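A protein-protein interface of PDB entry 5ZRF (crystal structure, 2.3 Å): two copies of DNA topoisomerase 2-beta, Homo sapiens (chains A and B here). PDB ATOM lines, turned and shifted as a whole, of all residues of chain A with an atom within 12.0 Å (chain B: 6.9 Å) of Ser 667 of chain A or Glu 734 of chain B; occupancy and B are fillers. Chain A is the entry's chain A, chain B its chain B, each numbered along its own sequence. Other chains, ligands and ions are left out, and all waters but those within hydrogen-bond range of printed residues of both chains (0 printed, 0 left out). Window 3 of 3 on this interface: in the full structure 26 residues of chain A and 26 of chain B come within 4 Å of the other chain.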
ATOM      1  N   PHE A 652       3.332   3.061 -18.041  1.00  0.00           N
ATOM      2  CA  PHE A 652       3.584   3.987 -16.943  1.00  0.00           C
ATOM      3  C   PHE A 652       2.284   4.476 -16.309  1.00  0.00           C
ATOM      4  O   PHE A 652       2.197   4.610 -15.083  1.00  0.00           O
ATOM      5  CB  PHE A 652       4.412   5.175 -17.435  1.00  0.00           C
ATOM      6  CG  PHE A 652       4.613   6.234 -16.391  1.00  0.00           C
ATOM      7  CD1 PHE A 652       3.703   7.277 -16.247  1.00  0.00           C
ATOM      8  CD2 PHE A 652       5.701   6.176 -15.535  1.00  0.00           C
ATOM      9  CE1 PHE A 652       3.883   8.248 -15.276  1.00  0.00           C
ATOM     10  CE2 PHE A 652       5.888   7.147 -14.564  1.00  0.00           C
ATOM     11  CZ  PHE A 652       4.976   8.182 -14.435  1.00  0.00           C
ATOM     12  N   ILE A 661       4.119   2.743  -9.056  1.00  0.00           N
ATOM     13  CA  ILE A 661       5.152   3.746  -9.286  1.00  0.00           C
ATOM     14  C   ILE A 661       4.616   5.091  -8.812  1.00  0.00           C
ATOM     15  O   ILE A 661       3.435   5.401  -8.997  1.00  0.00           O
ATOM     16  CB  ILE A 661       5.562   3.798 -10.777  1.00  0.00           C
ATOM     17  CG1 ILE A 661       6.576   4.898 -11.041  1.00  0.00           C
ATOM     18  CG2 ILE A 661       4.367   4.080 -11.662  1.00  0.00           C
ATOM     19  CD1 ILE A 661       7.442   4.597 -12.222  1.00  0.00           C
ATOM     20  N   THR A 662       5.482   5.880  -8.176  1.00  0.00           N
ATOM     21  CA  THR A 662       5.165   7.250  -7.790  1.00  0.00           C
ATOM     22  C   THR A 662       6.288   8.158  -8.262  1.00  0.00           C
ATOM     23  O   THR A 662       7.462   7.811  -8.125  1.00  0.00           O
ATOM     24  CB  THR A 662       4.993   7.399  -6.278  1.00  0.00           C
ATOM     25  OG1 THR A 662       6.242   7.133  -5.629  1.00  0.00           O
ATOM     26  CG2 THR A 662       3.935   6.445  -5.764  1.00  0.00           C
ATOM     27  N   ILE A 663       5.925   9.280  -8.886  1.00  0.00           N
ATOM     28  CA  ILE A 663       6.892  10.316  -9.220  1.00  0.00           C
ATOM     29  C   ILE A 663       6.886  11.472  -8.226  1.00  0.00           C
ATOM     30  O   ILE A 663       7.724  12.377  -8.340  1.00  0.00           O
ATOM     31  CB  ILE A 663       6.659  10.820 -10.656  1.00  0.00           C
ATOM     32  CG1 ILE A 663       5.361  11.614 -10.754  1.00  0.00           C
ATOM     33  CG2 ILE A 663       6.564   9.646 -11.600  1.00  0.00           C
ATOM     34  CD1 ILE A 663       5.007  12.008 -12.197  1.00  0.00           C
ATOM     35  N   GLU A 664       5.996  11.450  -7.235  1.00  0.00           N
ATOM     36  CA  GLU A 664       5.726  12.639  -6.432  1.00  0.00           C
ATOM     37  C   GLU A 664       6.950  13.069  -5.624  1.00  0.00           C
ATOM     38  O   GLU A 664       7.537  12.274  -4.885  1.00  0.00           O
ATOM     39  CB  GLU A 664       4.537  12.386  -5.499  1.00  0.00           C
ATOM     40  CG  GLU A 664       3.156  12.542  -6.161  1.00  0.00           C
ATOM     41  CD  GLU A 664       2.762  11.353  -7.036  1.00  0.00           C
ATOM     42  OE1 GLU A 664       3.614  10.460  -7.266  1.00  0.00           O
ATOM     43  OE2 GLU A 664       1.594  11.316  -7.496  1.00  0.00           O
ATOM     44  N   ASN A 665       7.331  14.337  -5.783  1.00  0.00           N
ATOM     45  CA  ASN A 665       8.419  14.965  -5.031  1.00  0.00           C
ATOM     46  C   ASN A 665       9.754  14.227  -5.197  1.00  0.00           C
ATOM     47  O   ASN A 665      10.615  14.259  -4.313  1.00  0.00           O
ATOM     48  CB  ASN A 665       8.054  15.093  -3.545  1.00  0.00           C
ATOM     49  CG  ASN A 665       8.951  16.072  -2.801  1.00  0.00           C
ATOM     50  OD1 ASN A 665       9.300  17.137  -3.326  1.00  0.00           O
ATOM     51  ND2 ASN A 665       9.334  15.709  -1.573  1.00  0.00           N
ATOM     52  N   ARG A 666       9.963  13.573  -6.331  1.00  0.00           N
ATOM     53  CA  ARG A 666      11.233  12.926  -6.621  1.00  0.00           C
ATOM     54  C   ARG A 666      12.056  13.801  -7.549  1.00  0.00           C
ATOM     55  O   ARG A 666      11.513  14.465  -8.433  1.00  0.00           O
ATOM     56  CB  ARG A 666      11.026  11.569  -7.276  1.00  0.00           C
ATOM     57  CG  ARG A 666      10.231  10.608  -6.459  1.00  0.00           C
ATOM     58  CD  ARG A 666       9.837   9.460  -7.339  1.00  0.00           C
ATOM     59  NE  ARG A 666       9.612   8.246  -6.573  1.00  0.00           N
ATOM     60  CZ  ARG A 666      10.517   7.288  -6.430  1.00  0.00           C
ATOM     61  NH1 ARG A 666      11.701   7.404  -7.016  1.00  0.00           N
ATOM     62  NH2 ARG A 666      10.232   6.213  -5.708  1.00  0.00           N
ATOM     63  N   SER A 667      13.370  13.794  -7.343  1.00  0.00           N
ATOM     64  CA  SER A 667      14.256  14.583  -8.180  1.00  0.00           C
ATOM     65  C   SER A 667      14.256  14.043  -9.602  1.00  0.00           C
ATOM     66  O   SER A 667      13.943  12.874  -9.855  1.00  0.00           O
ATOM     67  CB  SER A 667      15.678  14.577  -7.620  1.00  0.00           C
ATOM     68  OG  SER A 667      16.235  13.275  -7.652  1.00  0.00           O
ATOM     69  N   LYS A 668      14.604  14.921 -10.544  1.00  0.00           N
ATOM     70  CA  LYS A 668      14.692  14.506 -11.938  1.00  0.00           C
ATOM     71  C   LYS A 668      15.659  13.339 -12.107  1.00  0.00           C
ATOM     72  O   LYS A 668      15.341  12.356 -12.788  1.00  0.00           O
ATOM     73  CB  LYS A 668      15.108  15.694 -12.799  1.00  0.00           C
ATOM     74  CG  LYS A 668      15.208  15.405 -14.282  1.00  0.00           C
ATOM     75  CD  LYS A 668      15.535  16.678 -15.049  1.00  0.00           C
ATOM     76  CE  LYS A 668      15.759  16.393 -16.530  1.00  0.00           C
ATOM     77  NZ  LYS A 668      16.062  17.636 -17.296  1.00  0.00           N
ATOM     78  N   LYS A 669      16.834  13.413 -11.474  1.00  0.00           N
ATOM     79  CA  LYS A 669      17.808  12.327 -11.588  1.00  0.00           C
ATOM     80  C   LYS A 669      17.249  11.017 -11.042  1.00  0.00           C
ATOM     81  O   LYS A 669      17.334   9.974 -11.696  1.00  0.00           O
ATOM     82  CB  LYS A 669      19.105  12.695 -10.862  1.00  0.00           C
ATOM     83  CG  LYS A 669      19.957  13.731 -11.576  1.00  0.00           C
ATOM     84  N   ASP A 670      16.677  11.054  -9.839  1.00  0.00           N
ATOM     85  CA  ASP A 670      16.126   9.838  -9.247  1.00  0.00           C
ATOM     86  C   ASP A 670      15.019   9.251 -10.111  1.00  0.00           C
ATOM     87  O   ASP A 670      14.875   8.027 -10.206  1.00  0.00           O
ATOM     88  CB  ASP A 670      15.599  10.129  -7.844  1.00  0.00           C
ATOM     89  CG  ASP A 670      16.708  10.307  -6.838  1.00  0.00           C
ATOM     90  OD1 ASP A 670      17.854   9.913  -7.147  1.00  0.00           O
ATOM     91  OD2 ASP A 670      16.437  10.843  -5.741  1.00  0.00           O
ATOM     92  N   LEU A 671      14.217  10.109 -10.736  1.00  0.00           N
ATOM     93  CA  LEU A 671      13.107   9.616 -11.539  1.00  0.00           C
ATOM     94  C   LEU A 671      13.603   8.957 -12.819  1.00  0.00           C
ATOM     95  O   LEU A 671      13.110   7.891 -13.205  1.00  0.00           O
ATOM     96  CB  LEU A 671      12.147  10.764 -11.841  1.00  0.00           C
ATOM     97  CG  LEU A 671      10.952  10.453 -12.737  1.00  0.00           C
ATOM     98  CD1 LEU A 671      10.167   9.296 -12.171  1.00  0.00           C
ATOM     99  CD2 LEU A 671      10.069  11.672 -12.828  1.00  0.00           C
ATOM    100  N   ILE A 672      14.585   9.567 -13.487  1.00  0.00           N
ATOM    101  CA  ILE A 672      15.119   8.974 -14.709  1.00  0.00           C
ATOM    102  C   ILE A 672      15.813   7.658 -14.397  1.00  0.00           C
ATOM    103  O   ILE A 672      15.622   6.659 -15.102  1.00  0.00           O
ATOM    104  CB  ILE A 672      16.062   9.958 -15.427  1.00  0.00           C
ATOM    105  CG1 ILE A 672      15.288  11.186 -15.911  1.00  0.00           C
ATOM    106  CG2 ILE A 672      16.755   9.272 -16.596  1.00  0.00           C
ATOM    107  CD1 ILE A 672      16.143  12.202 -16.658  1.00  0.00           C
ATOM    108  N   GLN A 673      16.618   7.632 -13.329  1.00  0.00           N
ATOM    109  CA  GLN A 673      17.288   6.400 -12.924  1.00  0.00           C
ATOM    110  C   GLN A 673      16.277   5.295 -12.653  1.00  0.00           C
ATOM    111  O   GLN A 673      16.447   4.154 -13.102  1.00  0.00           O
ATOM    112  CB  GLN A 673      18.153   6.649 -11.685  1.00  0.00           C
ATOM    113  CG  GLN A 673      18.688   5.373 -11.025  1.00  0.00           C
ATOM    114  N   MET A 674      15.210   5.622 -11.923  1.00  0.00           N
ATOM    115  CA  MET A 674      14.214   4.610 -11.592  1.00  0.00           C
ATOM    116  C   MET A 674      13.513   4.106 -12.845  1.00  0.00           C
ATOM    117  O   MET A 674      13.300   2.897 -13.004  1.00  0.00           O
ATOM    118  CB  MET A 674      13.210   5.178 -10.592  1.00  0.00           C
ATOM    119  CG  MET A 674      12.212   4.163 -10.076  1.00  0.00           C
ATOM    120  SD  MET A 674      10.630   4.946  -9.764  1.00  0.00           S
ATOM    121  CE  MET A 674      10.474   5.864 -11.290  1.00  0.00           C
ATOM    122  N   LEU A 675      13.169   5.017 -13.760  1.00  0.00           N
ATOM    123  CA  LEU A 675      12.527   4.610 -15.005  1.00  0.00           C
ATOM    124  C   LEU A 675      13.425   3.679 -15.810  1.00  0.00           C
ATOM    125  O   LEU A 675      12.943   2.744 -16.458  1.00  0.00           O
ATOM    126  CB  LEU A 675      12.148   5.843 -15.826  1.00  0.00           C
ATOM    127  N   VAL A 676      14.739   3.905 -15.775  1.00  0.00           N
ATOM    128  CA  VAL A 676      15.645   2.984 -16.453  1.00  0.00           C
ATOM    129  C   VAL A 676      15.624   1.621 -15.774  1.00  0.00           C
ATOM    130  O   VAL A 676      15.507   0.583 -16.435  1.00  0.00           O
ATOM    131  CB  VAL A 676      17.072   3.556 -16.507  1.00  0.00           C
ATOM    132  CG1 VAL A 676      18.043   2.479 -17.007  1.00  0.00           C
ATOM    133  CG2 VAL A 676      17.120   4.785 -17.405  1.00  0.00           C
ATOM    134  N   PRO A 718      18.996   9.070 -21.722  1.00  0.00           N
ATOM    135  CA  PRO A 718      17.649   8.559 -22.016  1.00  0.00           C
ATOM    136  C   PRO A 718      16.612   9.671 -21.964  1.00  0.00           C
ATOM    137  O   PRO A 718      16.642  10.534 -21.081  1.00  0.00           O
ATOM    138  CB  PRO A 718      17.409   7.520 -20.913  1.00  0.00           C
ATOM    139  CG  PRO A 718      18.772   7.248 -20.314  1.00  0.00           C
ATOM    140  CD  PRO A 718      19.539   8.521 -20.470  1.00  0.00           C
ATOM    141  N   PHE A 720      12.818  10.406 -21.515  1.00  0.00           N
ATOM    142  CA  PHE A 720      11.510   9.994 -21.025  1.00  0.00           C
ATOM    143  C   PHE A 720      10.446  11.081 -21.163  1.00  0.00           C
ATOM    144  O   PHE A 720       9.344  10.924 -20.625  1.00  0.00           O
ATOM    145  CB  PHE A 720      11.637   9.486 -19.591  1.00  0.00           C
ATOM    146  CG  PHE A 720      12.478   8.231 -19.481  1.00  0.00           C
ATOM    147  CD1 PHE A 720      12.081   7.060 -20.116  1.00  0.00           C
ATOM    148  CD2 PHE A 720      13.661   8.222 -18.760  1.00  0.00           C
ATOM    149  CE1 PHE A 720      12.850   5.904 -20.034  1.00  0.00           C
ATOM    150  CE2 PHE A 720      14.435   7.067 -18.667  1.00  0.00           C
ATOM    151  CZ  PHE A 720      14.028   5.908 -19.306  1.00  0.00           C
ATOM    152  N   ASN A 721      10.778  12.209 -21.797  1.00  0.00           N
ATOM    153  CA  ASN A 721       9.834  13.318 -21.902  1.00  0.00           C
ATOM    154  C   ASN A 721       8.492  12.908 -22.502  1.00  0.00           C
ATOM    155  O   ASN A 721       7.454  13.462 -22.120  1.00  0.00           O
ATOM    156  CB  ASN A 721      10.448  14.450 -22.722  1.00  0.00           C
ATOM    157  CG  ASN A 721      11.466  15.250 -21.930  1.00  0.00           C
ATOM    158  OD1 ASN A 721      11.184  15.706 -20.822  1.00  0.00           O
ATOM    159  ND2 ASN A 721      12.669  15.399 -22.484  1.00  0.00           N
ATOM    160  N   LEU A 724       6.663  11.876 -19.257  1.00  0.00           N
ATOM    161  CA  LEU A 724       6.475  12.859 -18.197  1.00  0.00           C
ATOM    162  C   LEU A 724       5.878  14.180 -18.670  1.00  0.00           C
ATOM    163  O   LEU A 724       5.419  14.960 -17.824  1.00  0.00           O
ATOM    164  CB  LEU A 724       7.807  13.100 -17.496  1.00  0.00           C
ATOM    165  CG  LEU A 724       8.296  11.795 -16.854  1.00  0.00           C
ATOM    166  CD1 LEU A 724       9.717  11.912 -16.373  1.00  0.00           C
ATOM    167  CD2 LEU A 724       7.388  11.468 -15.685  1.00  0.00           C
ATOM    168  N   TRP B 729       5.699  16.060 -15.118  1.00  0.00           N
ATOM    169  CA  TRP B 729       6.915  16.679 -14.594  1.00  0.00           C
ATOM    170  C   TRP B 729       6.633  17.578 -13.393  1.00  0.00           C
ATOM    171  O   TRP B 729       7.475  17.699 -12.498  1.00  0.00           O
ATOM    172  CB  TRP B 729       7.597  17.518 -15.678  1.00  0.00           C
ATOM    173  CG  TRP B 729       8.551  16.799 -16.597  1.00  0.00           C
ATOM    174  CD1 TRP B 729       8.492  16.738 -17.972  1.00  0.00           C
ATOM    175  CD2 TRP B 729       9.726  16.077 -16.218  1.00  0.00           C
ATOM    176  NE1 TRP B 729       9.551  16.008 -18.458  1.00  0.00           N
ATOM    177  CE2 TRP B 729      10.324  15.594 -17.403  1.00  0.00           C
ATOM    178  CE3 TRP B 729      10.331  15.788 -14.991  1.00  0.00           C
ATOM    179  CZ2 TRP B 729      11.490  14.837 -17.393  1.00  0.00           C
ATOM    180  CZ3 TRP B 729      11.487  15.032 -14.984  1.00  0.00           C
ATOM    181  CH2 TRP B 729      12.054  14.568 -16.176  1.00  0.00           C
ATOM    182  N   SER B 730       5.463  18.227 -13.373  1.00  0.00           N
ATOM    183  CA  SER B 730       5.107  19.175 -12.322  1.00  0.00           C
ATOM    184  C   SER B 730       5.142  18.565 -10.931  1.00  0.00           C
ATOM    185  O   SER B 730       5.215  19.304  -9.949  1.00  0.00           O
ATOM    186  CB  SER B 730       3.710  19.730 -12.575  1.00  0.00           C
ATOM    187  OG  SER B 730       3.598  20.210 -13.895  1.00  0.00           O
ATOM    188  N   LEU B 731       5.058  17.246 -10.822  1.00  0.00           N
ATOM    189  CA  LEU B 731       5.075  16.578  -9.533  1.00  0.00           C
ATOM    190  C   LEU B 731       6.486  16.224  -9.081  1.00  0.00           C
ATOM    191  O   LEU B 731       6.643  15.632  -8.007  1.00  0.00           O
ATOM    192  CB  LEU B 731       4.213  15.305  -9.584  1.00  0.00           C
ATOM    193  CG  LEU B 731       2.782  15.440 -10.124  1.00  0.00           C
ATOM    194  CD1 LEU B 731       2.106  14.080 -10.244  1.00  0.00           C
ATOM    195  CD2 LEU B 731       1.951  16.382  -9.252  1.00  0.00           C
ATOM    196  N   THR B 732       7.511  16.544  -9.871  1.00  0.00           N
ATOM    197  CA  THR B 732       8.860  16.216  -9.442  1.00  0.00           C
ATOM    198  C   THR B 732       9.428  17.347  -8.594  1.00  0.00           C
ATOM    199  O   THR B 732       8.879  18.449  -8.535  1.00  0.00           O
ATOM    200  CB  THR B 732       9.767  15.934 -10.643  1.00  0.00           C
ATOM    201  OG1 THR B 732       9.970  17.135 -11.407  1.00  0.00           O
ATOM    202  CG2 THR B 732       9.145  14.863 -11.528  1.00  0.00           C
ATOM    203  N   LYS B 733      10.595  17.085  -7.999  1.00  0.00           N
ATOM    204  CA  LYS B 733      11.094  17.951  -6.938  1.00  0.00           C
ATOM    205  C   LYS B 733      11.428  19.339  -7.469  1.00  0.00           C
ATOM    206  O   LYS B 733      10.997  20.348  -6.904  1.00  0.00           O
ATOM    207  CB  LYS B 733      12.315  17.318  -6.270  1.00  0.00           C
ATOM    208  CG  LYS B 733      12.837  18.105  -5.074  1.00  0.00           C
ATOM    209  CD  LYS B 733      14.033  17.427  -4.421  1.00  0.00           C
ATOM    210  N   GLU B 734      12.176  19.407  -8.570  1.00  0.00           N
ATOM    211  CA  GLU B 734      12.595  20.701  -9.100  1.00  0.00           C
ATOM    212  C   GLU B 734      11.414  21.529  -9.591  1.00  0.00           C
ATOM    213  O   GLU B 734      11.434  22.759  -9.478  1.00  0.00           O
ATOM    214  CB  GLU B 734      13.600  20.505 -10.235  1.00  0.00           C
ATOM    215  CG  GLU B 734      14.913  19.891  -9.808  1.00  0.00           C
ATOM    216  CD  GLU B 734      14.835  18.388  -9.644  1.00  0.00           C
ATOM    217  OE1 GLU B 734      13.775  17.798  -9.947  1.00  0.00           O
ATOM    218  OE2 GLU B 734      15.842  17.796  -9.205  1.00  0.00           O
ATOM    219  N   LYS B 735      10.395  20.887 -10.152  1.00  0.00           N
ATOM    220  CA  LYS B 735       9.259  21.635 -10.670  1.00  0.00           C
ATOM    221  C   LYS B 735       8.348  22.128  -9.561  1.00  0.00           C
ATOM    222  O   LYS B 735       7.692  23.163  -9.725  1.00  0.00           O
ATOM    223  CB  LYS B 735       8.471  20.777 -11.656  1.00  0.00           C
ATOM    224  CG  LYS B 735       9.325  20.247 -12.773  1.00  0.00           C
ATOM    225  CD  LYS B 735       9.976  21.364 -13.573  1.00  0.00           C
ATOM    226  CE  LYS B 735       9.003  22.019 -14.536  1.00  0.00           C
ATOM    227  NZ  LYS B 735       9.724  22.890 -15.516  1.00  0.00           N
ATOM    228  N   VAL B 736       8.282  21.402  -8.441  1.00  0.00           N
ATOM    229  CA  VAL B 736       7.543  21.898  -7.288  1.00  0.00           C
ATOM    230  C   VAL B 736       8.182  23.179  -6.773  1.00  0.00           C
ATOM    231  O   VAL B 736       7.508  24.199  -6.588  1.00  0.00           O
ATOM    232  CB  VAL B 736       7.482  20.831  -6.183  1.00  0.00           C
ATOM    233  CG1 VAL B 736       6.938  21.454  -4.912  1.00  0.00           C
ATOM    234  CG2 VAL B 736       6.638  19.661  -6.606  1.00  0.00           C
ATOM    235  N   GLU B 737       9.497  23.140  -6.529  1.00  0.00           N
ATOM    236  CA  GLU B 737      10.205  24.328  -6.059  1.00  0.00           C
ATOM    237  C   GLU B 737      10.100  25.463  -7.067  1.00  0.00           C
ATOM    238  O   GLU B 737       9.956  26.631  -6.686  1.00  0.00           O
ATOM    239  CB  GLU B 737      11.672  23.999  -5.792  1.00  0.00           C
ATOM    240  CG  GLU B 737      11.905  22.928  -4.750  1.00  0.00           C
ATOM    241  CD  GLU B 737      13.302  22.333  -4.837  1.00  0.00           C
ATOM    242  OE1 GLU B 737      14.048  22.696  -5.775  1.00  0.00           O
ATOM    243  OE2 GLU B 737      13.647  21.492  -3.977  1.00  0.00           O
ATOM    244  N   GLU B 738      10.171  25.138  -8.360  1.00  0.00           N
ATOM    245  CA  GLU B 738      10.053  26.162  -9.390  1.00  0.00           C
ATOM    246  C   GLU B 738       8.677  26.817  -9.355  1.00  0.00           C
ATOM    247  O   GLU B 738       8.561  28.047  -9.355  1.00  0.00           O
ATOM    248  CB  GLU B 738      10.339  25.546 -10.761  1.00  0.00           C
ATOM    249  CG  GLU B 738      10.123  26.462 -11.951  1.00  0.00           C
ATOM    250  CD  GLU B 738      10.409  25.756 -13.278  1.00  0.00           C
ATOM    251  OE1 GLU B 738      10.928  24.621 -13.251  1.00  0.00           O
ATOM    252  OE2 GLU B 738      10.113  26.329 -14.346  1.00  0.00           O
ATOM    253  N   LEU B 739       7.620  26.007  -9.304  1.00  0.00           N
ATOM    254  CA  LEU B 739       6.265  26.548  -9.269  1.00  0.00           C
ATOM    255  C   LEU B 739       6.048  27.456  -8.059  1.00  0.00           C
ATOM    256  O   LEU B 739       5.408  28.506  -8.174  1.00  0.00           O
ATOM    257  CB  LEU B 739       5.253  25.407  -9.265  1.00  0.00           C
ATOM    258  CG  LEU B 739       3.790  25.835  -9.202  1.00  0.00           C
ATOM    259  CD1 LEU B 739       3.490  26.770 -10.365  1.00  0.00           C
ATOM    260  CD2 LEU B 739       2.889  24.620  -9.247  1.00  0.00           C
ATOM    261  N   LYS B 741       8.329  29.215  -6.406  1.00  0.00           N
ATOM    262  CA  LYS B 741       9.022  30.465  -6.710  1.00  0.00           C
ATOM    263  C   LYS B 741       8.218  31.317  -7.689  1.00  0.00           C
ATOM    264  O   LYS B 741       8.050  32.524  -7.484  1.00  0.00           O
ATOM    265  CB  LYS B 741      10.419  30.178  -7.267  1.00  0.00           C
ATOM    266  CG  LYS B 741      11.358  29.481  -6.298  1.00  0.00           C
ATOM    267  CD  LYS B 741      12.722  29.244  -6.934  1.00  0.00           C
ATOM    268  CE  LYS B 741      13.524  28.182  -6.179  1.00  0.00           C
ATOM    269  NZ  LYS B 741      13.741  28.554  -4.752  1.00  0.00           N
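Hydrophobic or aromatic side chains of chain A that line the printed part of chain B: Leu 671 and Leu 724.
O of Trp 729 of chain B sits at hydrogen-bond distance from OG1 of Thr 732 of chain B, at 2.8 Å.
The backbone carbonyl oxygen (O) of Thr 662 of chain A is in hydrogen-bond range of the guanidinium group (NE) of Arg 666 of chain A.
The side-chain carboxylate (OD2) of Asp 670 of chain A is in hydrogen-bond range of the side-chain hydroxyl (OG) of Ser 667 of chain A.
The backbone carbonyl oxygen (O) of Ile 663 of chain A sits close to the backbone carbonyl oxygen (O) of Leu 731 of chain B (3.4 Å).
OE1 of Glu 734 of chain B is in hydrogen-bond range of N of Lys 668 of chain A, at 3.1 Å.
O of Leu 724 of chain A lies within hydrogen-bond range of N of Trp 729 of chain B, at 2.9 Å.
The indole nitrogen of Trp 729 of chain B is in hydrogen-bond range of the side-chain amide oxygen of Asn 721 of chain A (2.9 Å).
The backbone carbonyl oxygen of Arg 666 of chain A is in hydrogen-bond range of the backbone NH of Lys 733 of chain B.
N of Asn 665 of chain A lies within hydrogen-bond range of O of Leu 731 of chain B, 2.7 Å away.
Glu 664 of chain A touches Leu 731 of chain B (CA to O, 3.5 Å).
CB of Thr 732 of chain B touches O of Arg 666 of chain A, at 3.2 Å.
Ser 667 of chain A touches Lys 733 of chain B (N to CB, 3.8 Å).
Ser 667 of chain A touches Glu 734 of chain B.
Lys 668 of chain A touches Trp 729 of chain B (CG to CH2, 3.8 Å).
Thr 732 of chain B touches Leu 671 of chain A (CG2 to CD2, 3.6 Å).
No position is printed for both chains.
Ser 667 of chain A touches just these residues of chain B: Lys 733 (3.8 Å) and Glu 734 (3.6 Å).
Of chain A, only Ser 667 and Lys 668 come within 4 Å of Glu 734 of chain B.
Thr 732 of chain B touches two residues of chain A.
Val 736 of chain B touches none of the printed residues of chain A.
No residue of chain A comes within 4 Å of Glu 738 of chain B.
Of the printed residues of chain B, Leu 671 of chain A touches Thr 732 (3.6 Å).
Of the printed residues of chain B, Asn 721 of chain A touches Trp 729 (2.9 Å).
The nearest residue of chain A that does not touch Glu 734 of chain B is Arg 666 of chain A (4.3 Å).
The nearest printed residue of chain B that does not touch Leu 724 of chain A is Ser 730 of chain B (5.5 Å).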
